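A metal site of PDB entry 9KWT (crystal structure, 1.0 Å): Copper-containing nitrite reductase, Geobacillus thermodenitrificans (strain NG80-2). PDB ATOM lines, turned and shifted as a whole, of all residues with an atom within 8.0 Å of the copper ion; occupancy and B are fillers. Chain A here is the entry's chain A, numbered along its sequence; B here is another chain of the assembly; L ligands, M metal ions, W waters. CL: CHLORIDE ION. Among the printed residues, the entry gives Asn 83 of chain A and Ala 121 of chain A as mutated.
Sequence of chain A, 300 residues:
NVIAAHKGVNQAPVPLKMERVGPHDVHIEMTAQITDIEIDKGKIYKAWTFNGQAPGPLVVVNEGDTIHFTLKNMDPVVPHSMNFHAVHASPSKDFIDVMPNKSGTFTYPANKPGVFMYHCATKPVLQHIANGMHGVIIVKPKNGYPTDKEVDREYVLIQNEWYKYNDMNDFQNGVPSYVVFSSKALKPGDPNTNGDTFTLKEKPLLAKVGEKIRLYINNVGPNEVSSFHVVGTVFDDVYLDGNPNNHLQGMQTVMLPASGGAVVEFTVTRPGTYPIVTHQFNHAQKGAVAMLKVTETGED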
ATOM      1  N   ASN A  83      -2.829 -13.928 -22.248  1.00  0.00           N
ATOM      2  CA  ASN A  83      -2.995 -13.735 -23.705  1.00  0.00           C
ATOM      3  C   ASN A  83      -2.946 -12.238 -23.936  1.00  0.00           C
ATOM      4  O   ASN A  83      -3.807 -11.521 -23.408  1.00  0.00           O
ATOM      5  CB  ASN A  83      -4.334 -14.331 -24.118  1.00  0.00           C
ATOM      6  CG  ASN A  83      -4.806 -13.952 -25.510  1.00  0.00           C
ATOM      7  OD1 ASN A  83      -4.375 -12.982 -26.112  1.00  0.00           O
ATOM      8  ND2 ASN A  83      -5.745 -14.738 -26.027  1.00  0.00           N
ATOM      9  N   PHE A  84      -1.928 -11.744 -24.630  1.00  0.00           N
ATOM     10  CA  PHE A  84      -1.896 -10.343 -25.049  1.00  0.00           C
ATOM     11  C   PHE A  84      -2.404 -10.266 -26.487  1.00  0.00           C
ATOM     12  O   PHE A  84      -1.818 -10.888 -27.379  1.00  0.00           O
ATOM     13  CB  PHE A  84      -0.467  -9.778 -25.048  1.00  0.00           C
ATOM     14  CG  PHE A  84       0.156  -9.590 -23.669  1.00  0.00           C
ATOM     15  CD1 PHE A  84      -0.151  -8.495 -22.879  1.00  0.00           C
ATOM     16  CD2 PHE A  84       1.118 -10.470 -23.202  1.00  0.00           C
ATOM     17  CE1 PHE A  84       0.449  -8.302 -21.654  1.00  0.00           C
ATOM     18  CE2 PHE A  84       1.720 -10.285 -21.966  1.00  0.00           C
ATOM     19  CZ  PHE A  84       1.381  -9.207 -21.201  1.00  0.00           C
ATOM     20  N   HIS A  85      -3.437  -9.459 -26.736  1.00  0.00           N
ATOM     21  CA  HIS A  85      -3.898  -9.293 -28.115  1.00  0.00           C
ATOM     22  C   HIS A  85      -2.887  -8.555 -28.978  1.00  0.00           C
ATOM     23  O   HIS A  85      -3.009  -8.567 -30.205  1.00  0.00           O
ATOM     24  CB  HIS A  85      -5.221  -8.527 -28.168  1.00  0.00           C
ATOM     25  CG  HIS A  85      -6.420  -9.330 -27.763  1.00  0.00           C
ATOM     26  ND1 HIS A  85      -7.687  -8.906 -28.066  1.00  0.00           N
ATOM     27  CD2 HIS A  85      -6.575 -10.506 -27.100  1.00  0.00           C
ATOM     28  CE1 HIS A  85      -8.569  -9.785 -27.625  1.00  0.00           C
ATOM     29  NE2 HIS A  85      -7.923 -10.775 -27.049  1.00  0.00           N
ATOM     30  N   PHE A  95       0.662 -19.117 -24.479  1.00  0.00           N
ATOM     31  CA  PHE A  95      -0.429 -18.618 -23.643  1.00  0.00           C
ATOM     32  C   PHE A  95      -0.916 -19.712 -22.692  1.00  0.00           C
ATOM     33  O   PHE A  95      -2.085 -19.725 -22.285  1.00  0.00           O
ATOM     34  CB  PHE A  95      -1.616 -18.098 -24.476  1.00  0.00           C
ATOM     35  CG  PHE A  95      -1.342 -16.907 -25.384  1.00  0.00           C
ATOM     36  CD1 PHE A  95      -0.217 -16.092 -25.286  1.00  0.00           C
ATOM     37  CD2 PHE A  95      -2.306 -16.572 -26.310  1.00  0.00           C
ATOM     38  CE1 PHE A  95      -0.066 -14.986 -26.138  1.00  0.00           C
ATOM     39  CE2 PHE A  95      -2.173 -15.471 -27.136  1.00  0.00           C
ATOM     40  CZ  PHE A  95      -1.064 -14.673 -27.049  1.00  0.00           C
ATOM     41  N   MET A 117      -6.451  -5.477 -25.858  1.00  0.00           N
ATOM     42  CA  MET A 117      -6.823  -6.174 -24.646  1.00  0.00           C
ATOM     43  C   MET A 117      -5.758  -7.216 -24.306  1.00  0.00           C
ATOM     44  O   MET A 117      -5.150  -7.809 -25.188  1.00  0.00           O
ATOM     45  CB  MET A 117      -8.240  -6.749 -24.766  1.00  0.00           C
ATOM     46  CG  MET A 117      -8.642  -7.699 -23.682  1.00  0.00           C
ATOM     47  SD  MET A 117     -10.334  -8.242 -23.951  1.00  0.00           S
ATOM     48  CE  MET A 117     -10.637  -9.170 -22.444  1.00  0.00           C
ATOM     49  N   TYR A 118      -5.581  -7.446 -23.015  1.00  0.00           N
ATOM     50  CA  TYR A 118      -4.930  -8.650 -22.524  1.00  0.00           C
ATOM     51  C   TYR A 118      -5.875  -9.321 -21.539  1.00  0.00           C
ATOM     52  O   TYR A 118      -6.751  -8.689 -20.948  1.00  0.00           O
ATOM     53  CB  TYR A 118      -3.542  -8.390 -21.938  1.00  0.00           C
ATOM     54  CG  TYR A 118      -3.447  -7.689 -20.588  1.00  0.00           C
ATOM     55  CD1 TYR A 118      -3.819  -8.316 -19.403  1.00  0.00           C
ATOM     56  CD2 TYR A 118      -2.902  -6.413 -20.494  1.00  0.00           C
ATOM     57  CE1 TYR A 118      -3.675  -7.685 -18.179  1.00  0.00           C
ATOM     58  CE2 TYR A 118      -2.749  -5.779 -19.260  1.00  0.00           C
ATOM     59  CZ  TYR A 118      -3.134  -6.424 -18.115  1.00  0.00           C
ATOM     60  OH  TYR A 118      -3.010  -5.870 -16.856  1.00  0.00           O
ATOM     61  N   HIS A 119      -5.681 -10.627 -21.350  1.00  0.00           N
ATOM     62  CA  HIS A 119      -6.556 -11.338 -20.436  1.00  0.00           C
ATOM     63  C   HIS A 119      -6.008 -12.736 -20.159  1.00  0.00           C
ATOM     64  O   HIS A 119      -5.198 -13.261 -20.917  1.00  0.00           O
ATOM     65  CB  HIS A 119      -7.985 -11.448 -21.015  1.00  0.00           C
ATOM     66  CG  HIS A 119      -8.049 -12.132 -22.341  1.00  0.00           C
ATOM     67  ND1 HIS A 119      -8.138 -13.495 -22.479  1.00  0.00           N
ATOM     68  CD2 HIS A 119      -8.070 -11.631 -23.605  1.00  0.00           C
ATOM     69  CE1 HIS A 119      -8.221 -13.801 -23.770  1.00  0.00           C
ATOM     70  NE2 HIS A 119      -8.162 -12.689 -24.473  1.00  0.00           N
ATOM     71  N   CYS A 120      -6.514 -13.345 -19.099  1.00  0.00           N
ATOM     72  CA  CYS A 120      -6.199 -14.735 -18.843  1.00  0.00           C
ATOM     73  C   CYS A 120      -6.827 -15.610 -19.932  1.00  0.00           C
ATOM     74  O   CYS A 120      -7.918 -15.327 -20.431  1.00  0.00           O
ATOM     75  CB  CYS A 120      -6.700 -15.110 -17.448  1.00  0.00           C
ATOM     76  SG  CYS A 120      -6.414 -16.828 -17.008  1.00  0.00           S
ATOM     77  N   ALA A 121      -6.109 -16.685 -20.276  1.00  0.00           N
ATOM     78  CA  ALA A 121      -6.443 -17.578 -21.369  1.00  0.00           C
ATOM     79  C   ALA A 121      -6.809 -18.978 -20.887  1.00  0.00           C
ATOM     80  O   ALA A 121      -6.850 -19.901 -21.705  1.00  0.00           O
ATOM     81  CB  ALA A 121      -5.275 -17.653 -22.370  1.00  0.00           C
ATOM     82  N   VAL A 125     -12.371 -19.665 -20.520  1.00  0.00           N
ATOM     83  CA  VAL A 125     -11.880 -18.306 -20.614  1.00  0.00           C
ATOM     84  C   VAL A 125     -12.931 -17.307 -20.122  1.00  0.00           C
ATOM     85  O   VAL A 125     -12.594 -16.314 -19.458  1.00  0.00           O
ATOM     86  CB  VAL A 125     -11.395 -18.004 -22.045  1.00  0.00           C
ATOM     87  CG1 VAL A 125     -10.997 -16.551 -22.203  1.00  0.00           C
ATOM     88  CG2 VAL A 125     -10.220 -18.917 -22.395  1.00  0.00           C
ATOM     89  N   ILE A 129     -12.025 -14.286 -17.480  1.00  0.00           N
ATOM     90  CA  ILE A 129     -12.252 -12.881 -17.813  1.00  0.00           C
ATOM     91  C   ILE A 129     -13.322 -12.286 -16.906  1.00  0.00           C
ATOM     92  O   ILE A 129     -13.122 -11.217 -16.312  1.00  0.00           O
ATOM     93  CB  ILE A 129     -12.623 -12.711 -19.304  1.00  0.00           C
ATOM     94  CG1 ILE A 129     -11.494 -13.193 -20.215  1.00  0.00           C
ATOM     95  CG2 ILE A 129     -12.923 -11.234 -19.576  1.00  0.00           C
ATOM     96  CD1 ILE A 129     -11.814 -13.082 -21.717  1.00  0.00           C
ATOM     97  N   VAL A 220     -13.203  -4.301 -22.653  1.00  0.00           N
ATOM     98  CA  VAL A 220     -12.748  -5.678 -22.460  1.00  0.00           C
ATOM     99  C   VAL A 220     -13.887  -6.673 -22.287  1.00  0.00           C
ATOM    100  O   VAL A 220     -13.646  -7.883 -22.277  1.00  0.00           O
ATOM    101  CB  VAL A 220     -11.724  -5.805 -21.318  1.00  0.00           C
ATOM    102  CG1 VAL A 220     -10.473  -4.968 -21.607  1.00  0.00           C
ATOM    103  CG2 VAL A 220     -12.335  -5.470 -19.967  1.00  0.00           C
ATOM    104  N   ALA A 258     -16.532  -6.362 -28.287  1.00  0.00           N
ATOM    105  CA  ALA A 258     -15.863  -6.908 -27.107  1.00  0.00           C
ATOM    106  C   ALA A 258     -14.409  -7.161 -27.457  1.00  0.00           C
ATOM    107  O   ALA A 258     -14.124  -7.838 -28.462  1.00  0.00           O
ATOM    108  CB  ALA A 258     -16.546  -8.201 -26.654  1.00  0.00           C
ATOM    109  N   SER A 259     -13.501  -6.610 -26.647  1.00  0.00           N
ATOM    110  CA  SER A 259     -12.050  -6.495 -26.819  1.00  0.00           C
ATOM    111  C   SER A 259     -11.637  -5.352 -27.727  1.00  0.00           C
ATOM    112  O   SER A 259     -10.429  -5.178 -27.970  1.00  0.00           O
ATOM    113  CB  SER A 259     -11.345  -7.782 -27.263  1.00  0.00           C
ATOM    114  OG  SER A 259     -11.545  -8.102 -28.623  1.00  0.00           O
ATOM    115  N   HIS B 229     -12.261 -12.512 -33.674  1.00  0.00           N
ATOM    116  CA  HIS B 229     -10.874 -12.418 -33.234  1.00  0.00           C
ATOM    117  C   HIS B 229     -10.171 -13.757 -33.429  1.00  0.00           C
ATOM    118  O   HIS B 229     -10.718 -14.806 -33.092  1.00  0.00           O
ATOM    119  CB  HIS B 229     -10.842 -12.029 -31.734  1.00  0.00           C
ATOM    120  CG  HIS B 229      -9.475 -12.037 -31.126  1.00  0.00           C
ATOM    121  ND1 HIS B 229      -8.586 -11.009 -31.335  1.00  0.00           N
ATOM    122  CD2 HIS B 229      -8.859 -12.905 -30.295  1.00  0.00           C
ATOM    123  CE1 HIS B 229      -7.460 -11.265 -30.693  1.00  0.00           C
ATOM    124  NE2 HIS B 229      -7.604 -12.407 -30.042  1.00  0.00           N
ATOM    125  N   VAL B 230      -8.932 -13.705 -33.927  1.00  0.00           N
ATOM    126  CA  VAL B 230      -8.053 -14.867 -33.990  1.00  0.00           C
ATOM    127  C   VAL B 230      -6.979 -14.711 -32.910  1.00  0.00           C
ATOM    128  O   VAL B 230      -6.231 -13.727 -32.882  1.00  0.00           O
ATOM    129  CB  VAL B 230      -7.438 -15.086 -35.379  1.00  0.00           C
ATOM    130  CG1 VAL B 230      -6.551 -16.321 -35.363  1.00  0.00           C
ATOM    131  CG2 VAL B 230      -8.534 -15.245 -36.420  1.00  0.00           C
ATOM    132  N   VAL B 231      -6.920 -15.685 -32.003  1.00  0.00           N
ATOM    133  CA  VAL B 231      -5.966 -15.673 -30.904  1.00  0.00           C
ATOM    134  C   VAL B 231      -4.543 -15.845 -31.439  1.00  0.00           C
ATOM    135  O   VAL B 231      -4.296 -16.681 -32.316  1.00  0.00           O
ATOM    136  CB  VAL B 231      -6.333 -16.797 -29.926  1.00  0.00           C
ATOM    137  CG1 VAL B 231      -5.352 -16.868 -28.770  1.00  0.00           C
ATOM    138  CG2 VAL B 231      -7.729 -16.607 -29.400  1.00  0.00           C
ATOM    139  N   GLY B 232      -3.600 -15.069 -30.894  1.00  0.00           N
ATOM    140  CA  GLY B 232      -2.200 -15.230 -31.244  1.00  0.00           C
ATOM    141  C   GLY B 232      -1.747 -14.497 -32.478  1.00  0.00           C
ATOM    142  O   GLY B 232      -0.601 -14.648 -32.900  1.00  0.00           O
ATOM    143  N   GLN B 252      -7.277  -5.888 -33.953  1.00  0.00           N
ATOM    144  CA  GLN B 252      -7.303  -7.076 -33.106  1.00  0.00           C
ATOM    145  C   GLN B 252      -8.579  -7.880 -33.303  1.00  0.00           C
ATOM    146  O   GLN B 252      -8.560  -9.116 -33.254  1.00  0.00           O
ATOM    147  CB  GLN B 252      -7.101  -6.720 -31.627  1.00  0.00           C
ATOM    148  CG  GLN B 252      -8.275  -6.039 -30.906  1.00  0.00           C
ATOM    149  CD  GLN B 252      -7.811  -5.437 -29.610  1.00  0.00           C
ATOM    150  OE1 GLN B 252      -7.395  -6.149 -28.684  1.00  0.00           O
ATOM    151  NE2 GLN B 252      -7.826  -4.110 -29.563  1.00  0.00           N
ATOM    152  N   THR B 253      -9.692  -7.173 -33.497  1.00  0.00           N
ATOM    153  CA  THR B 253     -11.035  -7.740 -33.452  1.00  0.00           C
ATOM    154  C   THR B 253     -11.891  -6.969 -34.431  1.00  0.00           C
ATOM    155  O   THR B 253     -11.797  -5.744 -34.492  1.00  0.00           O
ATOM    156  CB  THR B 253     -11.581  -7.643 -32.026  1.00  0.00           C
ATOM    157  OG1 THR B 253     -10.742  -8.469 -31.222  1.00  0.00           O
ATOM    158  CG2 THR B 253     -13.034  -8.119 -31.926  1.00  0.00           C
ATOM    159  N   VAL B 277     -12.457 -17.006 -32.359  1.00  0.00           N
ATOM    160  CA  VAL B 277     -13.583 -16.781 -31.459  1.00  0.00           C
ATOM    161  C   VAL B 277     -14.422 -15.606 -31.928  1.00  0.00           C
ATOM    162  O   VAL B 277     -13.964 -14.734 -32.666  1.00  0.00           O
ATOM    163  CB  VAL B 277     -13.115 -16.524 -30.007  1.00  0.00           C
ATOM    164  CG1 VAL B 277     -12.202 -17.635 -29.547  1.00  0.00           C
ATOM    165  CG2 VAL B 277     -12.414 -15.168 -29.852  1.00  0.00           C
ATOM    166  N   THR B 278     -15.665 -15.568 -31.431  1.00  0.00           N
ATOM    167  CA  THR B 278     -16.269 -14.275 -31.120  1.00  0.00           C
ATOM    168  C   THR B 278     -15.867 -13.922 -29.689  1.00  0.00           C
ATOM    169  O   THR B 278     -15.958 -14.754 -28.789  1.00  0.00           O
ATOM    170  CB  THR B 278     -17.789 -14.234 -31.311  1.00  0.00           C
ATOM    171  OG1 THR B 278     -18.210 -12.936 -30.875  1.00  0.00           O
ATOM    172  CG2 THR B 278     -18.511 -15.317 -30.534  1.00  0.00           C
ATOM    173  N   HIS B 279     -15.379 -12.701 -29.519  1.00  0.00           N
ATOM    174  CA  HIS B 279     -14.850 -12.268 -28.222  1.00  0.00           C
ATOM    175  C   HIS B 279     -15.939 -11.844 -27.255  1.00  0.00           C
ATOM    176  O   HIS B 279     -15.613 -11.456 -26.127  1.00  0.00           O
ATOM    177  CB  HIS B 279     -13.818 -11.154 -28.408  1.00  0.00           C
ATOM    178  CG  HIS B 279     -12.637 -11.308 -27.508  1.00  0.00           C
ATOM    179  ND1 HIS B 279     -12.669 -11.004 -26.171  1.00  0.00           N
ATOM    180  CD2 HIS B 279     -11.396 -11.758 -27.763  1.00  0.00           C
ATOM    181  CE1 HIS B 279     -11.480 -11.282 -25.639  1.00  0.00           C
ATOM    182  NE2 HIS B 279     -10.695 -11.746 -26.590  1.00  0.00           N
ATOM    183  N   PHE B 281     -17.702 -13.358 -24.925  1.00  0.00           N
ATOM    184  CA  PHE B 281     -17.271 -14.671 -24.451  1.00  0.00           C
ATOM    185  C   PHE B 281     -18.409 -15.550 -23.953  1.00  0.00           C
ATOM    186  O   PHE B 281     -18.227 -16.765 -23.864  1.00  0.00           O
ATOM    187  CB  PHE B 281     -16.087 -14.568 -23.460  1.00  0.00           C
ATOM    188  CG  PHE B 281     -14.810 -15.020 -24.095  1.00  0.00           C
ATOM    189  CD1 PHE B 281     -14.524 -16.376 -24.161  1.00  0.00           C
ATOM    190  CD2 PHE B 281     -13.960 -14.133 -24.741  1.00  0.00           C
ATOM    191  CE1 PHE B 281     -13.406 -16.827 -24.847  1.00  0.00           C
ATOM    192  CE2 PHE B 281     -12.847 -14.581 -25.415  1.00  0.00           C
ATOM    193  CZ  PHE B 281     -12.568 -15.926 -25.479  1.00  0.00           C
HETATM  194 CL    CL L   1      -9.187 -14.423 -27.006  1.00  0.00          CL
HETATM  195 CU    CU M   1      -8.833 -12.410 -26.358  1.00  0.00          CU
HETATM  196  O   HOH W   1      -7.003 -13.486 -27.581  1.00  0.00           O
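The copper ion is bound by a ring nitrogen (NE2) of His 279 of chain B (2.0 Å), a ring nitrogen (NE2) of His 85 (2.0 Å), a ring nitrogen (NE2) of His 119 (2.0 Å), a chlorine (CL) of the ligand (2.1 Å) and water W1 (2.4 Å).
A ring nitrogen (NE2) of His 229 of chain B lies close to a ring nitrogen (NE2) of His 85 (3.4 Å).
N of His 85 lies within hydrogen-bond range of O of Met 117, 2.8 Å away.
The side-chain amide oxygen (OE1) of Gln 252 of chain B lies within hydrogen-bond range of a ring nitrogen (ND1) of His 85 (2.8 Å).
The backbone carbonyl oxygen of His 119 is in hydrogen-bond range of the backbone NH of Asn 83 (2.8 Å).
N of Val 277 of chain B is in hydrogen-bond range of O of His 229 of chain B (2.9 Å).
ND1 of His 229 of chain B lies within hydrogen-bond range of OG1 of Thr 253 of chain B.
O of Gln 252 of chain B sits at hydrogen-bond distance from ND1 of His 229 of chain B (2.7 Å).
Water W1 lies within hydrogen-bond range of NE2 of His 229 of chain B (2.8 Å) and OD1 of Asn 83 (3.1 Å).
Residues that only touch the copper ion: Asn 83 and His 229 of chain B.
Of the 24 residues printed, 5 come within 4 Å of the copper ion.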
